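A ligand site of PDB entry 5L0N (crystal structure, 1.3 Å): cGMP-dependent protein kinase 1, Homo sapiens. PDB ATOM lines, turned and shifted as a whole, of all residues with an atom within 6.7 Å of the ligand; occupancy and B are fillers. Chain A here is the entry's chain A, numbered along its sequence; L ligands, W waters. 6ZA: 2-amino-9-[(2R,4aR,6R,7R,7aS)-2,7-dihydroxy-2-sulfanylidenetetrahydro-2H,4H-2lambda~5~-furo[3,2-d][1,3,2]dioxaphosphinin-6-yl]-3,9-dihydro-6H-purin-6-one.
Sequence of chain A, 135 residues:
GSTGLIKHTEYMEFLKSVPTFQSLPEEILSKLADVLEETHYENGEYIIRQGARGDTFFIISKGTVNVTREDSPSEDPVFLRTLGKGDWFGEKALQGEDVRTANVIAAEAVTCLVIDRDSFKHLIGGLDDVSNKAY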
ATOM      1  N   ILE A  48      27.651  22.545   7.866  1.00  0.00           N
ATOM      2  CA  ILE A  48      28.275  23.866   7.840  1.00  0.00           C
ATOM      3  C   ILE A  48      29.773  23.668   8.074  1.00  0.00           C
ATOM      4  O   ILE A  48      30.176  22.896   8.959  1.00  0.00           O
ATOM      5  CB  ILE A  48      27.702  24.775   8.932  1.00  0.00           C
ATOM      6  CG1 ILE A  48      26.240  25.121   8.612  1.00  0.00           C
ATOM      7  CG2 ILE A  48      28.562  26.042   9.104  1.00  0.00           C
ATOM      8  CD1 ILE A  48      25.572  25.990   9.656  1.00  0.00           C
ATOM      9  N   GLY A  54      27.717  31.510   4.250  1.00  0.00           N
ATOM     10  CA  GLY A  54      26.470  30.869   3.904  1.00  0.00           C
ATOM     11  C   GLY A  54      25.286  31.717   4.287  1.00  0.00           C
ATOM     12  O   GLY A  54      25.394  32.724   4.993  1.00  0.00           O
ATOM     13  N   THR A  56      22.064  29.964   4.954  1.00  0.00           N
ATOM     14  CA  THR A  56      21.036  29.021   5.334  1.00  0.00           C
ATOM     15  C   THR A  56      21.021  28.758   6.846  1.00  0.00           C
ATOM     16  O   THR A  56      22.052  28.719   7.526  1.00  0.00           O
ATOM     17  CB  THR A  56      21.220  27.708   4.570  1.00  0.00           C
ATOM     18  OG1 THR A  56      22.594  27.326   4.621  1.00  0.00           O
ATOM     19  CG2 THR A  56      20.783  27.858   3.116  1.00  0.00           C
ATOM     20  N   VAL A  67      28.848  19.918  16.802  1.00  0.00           N
ATOM     21  CA  VAL A  67      29.283  21.294  16.572  1.00  0.00           C
ATOM     22  C   VAL A  67      30.713  21.353  17.066  1.00  0.00           C
ATOM     23  O   VAL A  67      30.989  21.017  18.220  1.00  0.00           O
ATOM     24  CB  VAL A  67      28.410  22.306  17.340  1.00  0.00           C
ATOM     25  CG1 VAL A  67      28.878  23.730  17.047  1.00  0.00           C
ATOM     26  CG2 VAL A  67      26.944  22.123  17.002  1.00  0.00           C
ATOM     27  N   THR A  68      31.620  21.755  16.192  1.00  0.00           N
ATOM     28  CA  THR A  68      33.033  21.855  16.544  1.00  0.00           C
ATOM     29  C   THR A  68      33.564  23.191  16.056  1.00  0.00           C
ATOM     30  O   THR A  68      32.966  23.824  15.191  1.00  0.00           O
ATOM     31  CB  THR A  68      33.860  20.715  15.962  1.00  0.00           C
ATOM     32  OG1 THR A  68      34.057  20.931  14.567  1.00  0.00           O
ATOM     33  CG2 THR A  68      33.181  19.357  16.203  1.00  0.00           C
ATOM     34  N   ARG A  69      34.687  23.634  16.610  1.00  0.00           N
ATOM     35  CA  ARG A  69      35.215  24.944  16.250  1.00  0.00           C
ATOM     36  C   ARG A  69      36.717  24.949  16.423  1.00  0.00           C
ATOM     37  O   ARG A  69      37.240  24.443  17.416  1.00  0.00           O
ATOM     38  CB  ARG A  69      34.591  26.020  17.152  1.00  0.00           C
ATOM     39  CG  ARG A  69      34.983  27.456  16.799  1.00  0.00           C
ATOM     40  CD  ARG A  69      34.859  28.375  18.022  1.00  0.00           C
ATOM     41  NE  ARG A  69      35.854  28.028  19.040  1.00  0.00           N
ATOM     42  CZ  ARG A  69      35.590  27.722  20.311  1.00  0.00           C
ATOM     43  NH1 ARG A  69      34.342  27.715  20.773  1.00  0.00           N
ATOM     44  NH2 ARG A  69      36.581  27.417  21.125  1.00  0.00           N
ATOM     45  N   LEU A  80      32.335  21.132  20.663  1.00  0.00           N
ATOM     46  CA  LEU A  80      31.542  22.025  21.497  1.00  0.00           C
ATOM     47  C   LEU A  80      30.312  21.328  22.052  1.00  0.00           C
ATOM     48  O   LEU A  80      30.121  21.292  23.271  1.00  0.00           O
ATOM     49  CB  LEU A  80      31.150  23.291  20.729  1.00  0.00           C
ATOM     50  CG  LEU A  80      32.309  24.113  20.186  1.00  0.00           C
ATOM     51  CD1 LEU A  80      31.769  25.382  19.503  1.00  0.00           C
ATOM     52  CD2 LEU A  80      33.349  24.434  21.270  1.00  0.00           C
ATOM     53  N   ARG A  81      29.451  20.800  21.192  1.00  0.00           N
ATOM     54  CA  ARG A  81      28.221  20.204  21.686  1.00  0.00           C
ATOM     55  C   ARG A  81      27.599  19.342  20.604  1.00  0.00           C
ATOM     56  O   ARG A  81      27.929  19.462  19.413  1.00  0.00           O
ATOM     57  CB  ARG A  81      27.208  21.295  22.092  1.00  0.00           C
ATOM     58  CG  ARG A  81      26.551  21.991  20.892  1.00  0.00           C
ATOM     59  CD  ARG A  81      25.723  23.203  21.318  1.00  0.00           C
ATOM     60  NE  ARG A  81      26.550  24.351  21.626  1.00  0.00           N
ATOM     61  CZ  ARG A  81      26.808  24.795  22.850  1.00  0.00           C
ATOM     62  NH1 ARG A  81      26.314  24.188  23.932  1.00  0.00           N
ATOM     63  NH2 ARG A  81      27.574  25.871  23.001  1.00  0.00           N
ATOM     64  N   LEU A  83      23.875  18.427  18.876  1.00  0.00           N
ATOM     65  CA  LEU A  83      22.503  18.867  18.671  1.00  0.00           C
ATOM     66  C   LEU A  83      21.711  17.730  18.042  1.00  0.00           C
ATOM     67  O   LEU A  83      22.269  16.919  17.295  1.00  0.00           O
ATOM     68  CB  LEU A  83      22.420  20.145  17.804  1.00  0.00           C
ATOM     69  CG  LEU A  83      23.123  21.361  18.399  1.00  0.00           C
ATOM     70  CD1 LEU A  83      23.156  22.510  17.382  1.00  0.00           C
ATOM     71  CD2 LEU A  83      22.448  21.805  19.693  1.00  0.00           C
ATOM     72  N   TRP A  88      18.459  23.496  16.310  1.00  0.00           N
ATOM     73  CA  TRP A  88      18.663  24.320  15.122  1.00  0.00           C
ATOM     74  C   TRP A  88      20.056  24.937  15.194  1.00  0.00           C
ATOM     75  O   TRP A  88      20.716  24.927  16.242  1.00  0.00           O
ATOM     76  CB  TRP A  88      17.576  25.421  15.054  1.00  0.00           C
ATOM     77  CG  TRP A  88      17.657  26.286  16.266  1.00  0.00           C
ATOM     78  CD1 TRP A  88      18.458  27.372  16.439  1.00  0.00           C
ATOM     79  CD2 TRP A  88      16.938  26.121  17.494  1.00  0.00           C
ATOM     80  NE1 TRP A  88      18.320  27.865  17.707  1.00  0.00           N
ATOM     81  CE2 TRP A  88      17.373  27.140  18.372  1.00  0.00           C
ATOM     82  CE3 TRP A  88      15.977  25.215  17.940  1.00  0.00           C
ATOM     83  CZ2 TRP A  88      16.898  27.261  19.668  1.00  0.00           C
ATOM     84  CZ3 TRP A  88      15.486  25.355  19.237  1.00  0.00           C
ATOM     85  CH2 TRP A  88      15.956  26.369  20.078  1.00  0.00           C
ATOM     86  N   PHE A  89      20.479  25.501  14.067  1.00  0.00           N
ATOM     87  CA  PHE A  89      21.782  26.138  13.998  1.00  0.00           C
ATOM     88  C   PHE A  89      21.861  27.008  12.755  1.00  0.00           C
ATOM     89  O   PHE A  89      21.135  26.774  11.775  1.00  0.00           O
ATOM     90  CB  PHE A  89      22.941  25.113  14.040  1.00  0.00           C
ATOM     91  CG  PHE A  89      22.835  23.997  13.041  1.00  0.00           C
ATOM     92  CD1 PHE A  89      22.186  22.809  13.358  1.00  0.00           C
ATOM     93  CD2 PHE A  89      23.374  24.135  11.782  1.00  0.00           C
ATOM     94  CE1 PHE A  89      22.101  21.788  12.430  1.00  0.00           C
ATOM     95  CE2 PHE A  89      23.318  23.122  10.861  1.00  0.00           C
ATOM     96  CZ  PHE A  89      22.673  21.942  11.180  1.00  0.00           C
ATOM     97  N   GLY A  90      22.696  28.033  12.808  1.00  0.00           N
ATOM     98  CA  GLY A  90      22.923  28.907  11.682  1.00  0.00           C
ATOM     99  C   GLY A  90      21.998  30.101  11.573  1.00  0.00           C
ATOM    100  O   GLY A  90      21.989  30.764  10.538  1.00  0.00           O
ATOM    101  N   GLU A  91      21.261  30.426  12.640  1.00  0.00           N
ATOM    102  CA  GLU A  91      20.204  31.415  12.509  1.00  0.00           C
ATOM    103  C   GLU A  91      20.747  32.779  12.099  1.00  0.00           C
ATOM    104  O   GLU A  91      20.081  33.486  11.332  1.00  0.00           O
ATOM    105  CB  GLU A  91      19.389  31.524  13.802  1.00  0.00           C
ATOM    106  CG  GLU A  91      18.001  32.139  13.621  1.00  0.00           C
ATOM    107  CD  GLU A  91      18.031  33.647  13.368  1.00  0.00           C
ATOM    108  OE1 GLU A  91      18.946  34.325  13.880  1.00  0.00           O
ATOM    109  OE2 GLU A  91      17.154  34.147  12.636  1.00  0.00           O
ATOM    110  N   LYS A  92      21.928  33.171  12.572  1.00  0.00           N
ATOM    111  CA  LYS A  92      22.365  34.535  12.261  1.00  0.00           C
ATOM    112  C   LYS A  92      22.563  34.745  10.771  1.00  0.00           C
ATOM    113  O   LYS A  92      22.521  35.896  10.323  1.00  0.00           O
ATOM    114  CB  LYS A  92      23.630  34.903  13.048  1.00  0.00           C
ATOM    115  CG  LYS A  92      24.864  34.216  12.552  1.00  0.00           C
ATOM    116  CD  LYS A  92      26.075  34.630  13.388  1.00  0.00           C
ATOM    117  CE  LYS A  92      27.340  33.918  12.924  1.00  0.00           C
ATOM    118  NZ  LYS A  92      27.736  34.392  11.568  1.00  0.00           N
ATOM    119  N   ALA A  93      22.700  33.668   9.997  1.00  0.00           N
ATOM    120  CA  ALA A  93      22.807  33.815   8.557  1.00  0.00           C
ATOM    121  C   ALA A  93      21.541  34.424   7.967  1.00  0.00           C
ATOM    122  O   ALA A  93      21.600  35.070   6.916  1.00  0.00           O
ATOM    123  CB  ALA A  93      23.085  32.451   7.914  1.00  0.00           C
ATOM    124  N   GLU A  97      24.455  37.694   8.587  1.00  0.00           N
ATOM    125  CA  GLU A  97      25.748  37.437   9.200  1.00  0.00           C
ATOM    126  C   GLU A  97      26.230  36.095   8.674  1.00  0.00           C
ATOM    127  O   GLU A  97      26.047  35.032   9.286  1.00  0.00           O
ATOM    128  CB  GLU A  97      25.636  37.431  10.718  1.00  0.00           C
ATOM    129  CG  GLU A  97      24.998  38.684  11.300  1.00  0.00           C
ATOM    130  CD  GLU A  97      25.831  39.932  11.088  1.00  0.00           C
ATOM    131  OE1 GLU A  97      26.996  39.822  10.646  1.00  0.00           O
ATOM    132  OE2 GLU A  97      25.309  41.032  11.367  1.00  0.00           O
ATOM    133  N   ASP A  98      26.850  36.145   7.492  1.00  0.00           N
ATOM    134  CA  ASP A  98      27.069  34.942   6.689  1.00  0.00           C
ATOM    135  C   ASP A  98      28.358  34.191   7.023  1.00  0.00           C
ATOM    136  O   ASP A  98      28.547  33.085   6.521  1.00  0.00           O
ATOM    137  CB  ASP A  98      26.977  35.244   5.191  1.00  0.00           C
ATOM    138  CG  ASP A  98      28.106  36.135   4.663  1.00  0.00           C
ATOM    139  OD1 ASP A  98      28.939  36.651   5.423  1.00  0.00           O
ATOM    140  OD2 ASP A  98      28.147  36.357   3.429  1.00  0.00           O
ATOM    141  N   VAL A  99      29.221  34.733   7.873  1.00  0.00           N
ATOM    142  CA  VAL A  99      30.467  34.044   8.191  1.00  0.00           C
ATOM    143  C   VAL A  99      30.190  32.887   9.146  1.00  0.00           C
ATOM    144  O   VAL A  99      29.722  33.093  10.268  1.00  0.00           O
ATOM    145  CB  VAL A  99      31.468  35.013   8.825  1.00  0.00           C
ATOM    146  CG1 VAL A  99      32.721  34.270   9.267  1.00  0.00           C
ATOM    147  CG2 VAL A  99      31.808  36.116   7.863  1.00  0.00           C
ATOM    148  N   ARG A 100      30.468  31.655   8.714  1.00  0.00           N
ATOM    149  CA  ARG A 100      30.231  30.499   9.565  1.00  0.00           C
ATOM    150  C   ARG A 100      31.313  30.418  10.634  1.00  0.00           C
ATOM    151  O   ARG A 100      32.502  30.383  10.325  1.00  0.00           O
ATOM    152  CB  ARG A 100      30.201  29.206   8.747  1.00  0.00           C
ATOM    153  CG  ARG A 100      29.145  29.201   7.649  1.00  0.00           C
ATOM    154  CD  ARG A 100      27.719  29.399   8.161  1.00  0.00           C
ATOM    155  NE  ARG A 100      26.761  28.904   7.167  1.00  0.00           N
ATOM    156  CZ  ARG A 100      25.444  28.903   7.312  1.00  0.00           C
ATOM    157  NH1 ARG A 100      24.870  29.395   8.398  1.00  0.00           N
ATOM    158  NH2 ARG A 100      24.689  28.402   6.341  1.00  0.00           N
ATOM    159  N   THR A 101      30.895  30.414  11.898  1.00  0.00           N
ATOM    160  CA  THR A 101      31.814  30.491  13.027  1.00  0.00           C
ATOM    161  C   THR A 101      32.119  29.145  13.669  1.00  0.00           C
ATOM    162  O   THR A 101      32.935  29.083  14.592  1.00  0.00           O
ATOM    163  CB  THR A 101      31.275  31.434  14.104  1.00  0.00           C
ATOM    164  OG1 THR A 101      30.102  30.881  14.706  1.00  0.00           O
ATOM    165  CG2 THR A 101      30.975  32.805  13.524  1.00  0.00           C
ATOM    166  N   ALA A 102      31.519  28.076  13.185  1.00  0.00           N
ATOM    167  CA  ALA A 102      31.772  26.746  13.710  1.00  0.00           C
ATOM    168  C   ALA A 102      31.419  25.749  12.623  1.00  0.00           C
ATOM    169  O   ALA A 102      30.676  26.072  11.682  1.00  0.00           O
ATOM    170  CB  ALA A 102      30.936  26.464  14.948  1.00  0.00           C
ATOM    171  N   ASN A 103      31.937  24.534  12.758  1.00  0.00           N
ATOM    172  CA  ASN A 103      31.552  23.420  11.914  1.00  0.00           C
ATOM    173  C   ASN A 103      30.344  22.743  12.519  1.00  0.00           C
ATOM    174  O   ASN A 103      30.234  22.629  13.743  1.00  0.00           O
ATOM    175  CB  ASN A 103      32.672  22.382  11.872  1.00  0.00           C
ATOM    176  CG  ASN A 103      33.989  22.972  11.516  1.00  0.00           C
ATOM    177  OD1 ASN A 103      34.183  23.449  10.411  1.00  0.00           O
ATOM    178  ND2 ASN A 103      34.927  22.954  12.469  1.00  0.00           N
ATOM    179  N   VAL A 104      29.425  22.276  11.668  1.00  0.00           N
ATOM    180  CA  VAL A 104      28.336  21.425  12.114  1.00  0.00           C
ATOM    181  C   VAL A 104      28.355  20.194  11.244  1.00  0.00           C
ATOM    182  O   VAL A 104      28.203  20.290  10.019  1.00  0.00           O
ATOM    183  CB  VAL A 104      26.969  22.120  12.051  1.00  0.00           C
ATOM    184  CG1 VAL A 104      25.928  21.217  12.623  1.00  0.00           C
ATOM    185  CG2 VAL A 104      27.027  23.430  12.803  1.00  0.00           C
HETATM  186  N12 6ZA L   1      29.780  28.270  19.105  1.00  0.00           N
HETATM  187  C15 6ZA L   1      26.557  27.324  13.760  1.00  0.00           C
HETATM  188  C17 6ZA L   1      25.903  26.942  15.957  1.00  0.00           C
HETATM  189  C20 6ZA L   1      25.950  25.907  18.090  1.00  0.00           C
HETATM  190  C21 6ZA L   1      27.725  26.834  18.898  1.00  0.00           C
HETATM  191  C22 6ZA L   1      28.917  27.344  19.720  1.00  0.00           C
HETATM  192  S01 6ZA L   1      26.006  31.074  10.956  1.00  0.00           S
HETATM  193  P02 6ZA L   1      26.929  30.047  12.259  1.00  0.00           P
HETATM  194  O03 6ZA L   1      26.787  26.507  14.736  1.00  0.00           O
HETATM  195  O04 6ZA L   1      25.908  29.770  13.594  1.00  0.00           O
HETATM  196  O05 6ZA L   1      27.179  28.441  11.649  1.00  0.00           O
HETATM  197  O06 6ZA L   1      24.168  28.598  15.207  1.00  0.00           O
HETATM  198  O07 6ZA L   1      28.311  30.582  12.835  1.00  0.00           O
HETATM  199  O08 6ZA L   1      29.117  27.005  20.860  1.00  0.00           O
HETATM  200  N09 6ZA L   1      26.470  26.715  17.104  1.00  0.00           N
HETATM  201  N10 6ZA L   1      28.456  28.243  16.982  1.00  0.00           N
HETATM  202  N11 6ZA L   1      26.738  25.980  19.183  1.00  0.00           N
HETATM  203  N13 6ZA L   1      30.471  29.638  17.164  1.00  0.00           N
HETATM  204  C14 6ZA L   1      26.329  28.815  14.552  1.00  0.00           C
HETATM  205  C16 6ZA L   1      25.583  28.514  15.587  1.00  0.00           C
HETATM  206  C18 6ZA L   1      27.609  27.434  12.685  1.00  0.00           C
HETATM  207  C19 6ZA L   1      27.547  27.288  17.615  1.00  0.00           C
HETATM  208  C23 6ZA L   1      29.564  28.716  17.763  1.00  0.00           C
HETATM  209  O   HOH W   1      30.879  28.430  22.600  1.00  0.00           O
HETATM  210  O   HOH W   2      23.731  31.680  14.407  1.00  0.00           O
HETATM  211  O   HOH W   3      22.771  26.206  17.519  1.00  0.00           O
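NZ of Lys 92 lies close to S01 of the ligand, 3.8 Å away. An oxygen (O08) of the ligand is in hydrogen-bond range of the guanidinium group (NH2) of Arg 81, at 2.9 Å. A sulfur (S01) of the ligand lies close to the guanidinium group (NH1) of Arg 100, 3.3 Å away. The side-chain hydroxyl (OG1) of Thr 101 sits at hydrogen-bond distance from an oxygen (O07) of the ligand. The backbone NH (N) of Gly 90 sits at hydrogen-bond distance from an oxygen (O06) of the ligand, at 2.9 Å. The backbone NH of Thr 101 is in hydrogen-bond range of an oxygen (O07) of the ligand, 2.8 Å away.
O of Arg 81 is in hydrogen-bond range of N of Val 67. The guanidinium group of Arg 100 sits at hydrogen-bond distance from the backbone carbonyl oxygen of Thr 56, 2.9 Å away. The side-chain amino group (NZ) of Lys 92 lies within hydrogen-bond range of the backbone carbonyl oxygen (O) of Glu 97, 2.9 Å away. O of Ile 48 sits at hydrogen-bond distance from N of Val 104, at 2.9 Å. N of Leu 80 lies within hydrogen-bond range of O of Val 67 (2.8 Å). NZ of Lys 92 lies within hydrogen-bond range of O of Val 99 (2.7 Å).
Ile 48 touches the ligand. Val 67 touches the ligand (CG1 to N11, 3.8 Å). CD1 of Leu 80 touches O08 of the ligand, 3.4 Å away. Phe 89 touches the ligand (CA to O06, 3.6 Å). Val 99 touches the ligand (O to O07, 3.9 Å). Ala 102 touches the ligand. CG2 of Val 104 touches O03 of the ligand (3.6 Å). Hydrophobic or aromatic side chains that line the ligand: Ile 48, Val 67, Leu 80, Phe 89, Ala 102 and Val 104. Of the 23 residues printed, 12 come within 4 Å of the ligand. Along chain A the residues within 4 Å of the ligand span positions 48 to 104. The nearest printed residue that does not touch the ligand is Glu 91 (4.3 Å).
Water W2 lies within hydrogen-bond range of the backbone NH of Lys 92 (3.0 Å), an oxygen (O04) of the ligand (3.0 Å) and the backbone NH of Glu 91 (3.3 Å).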
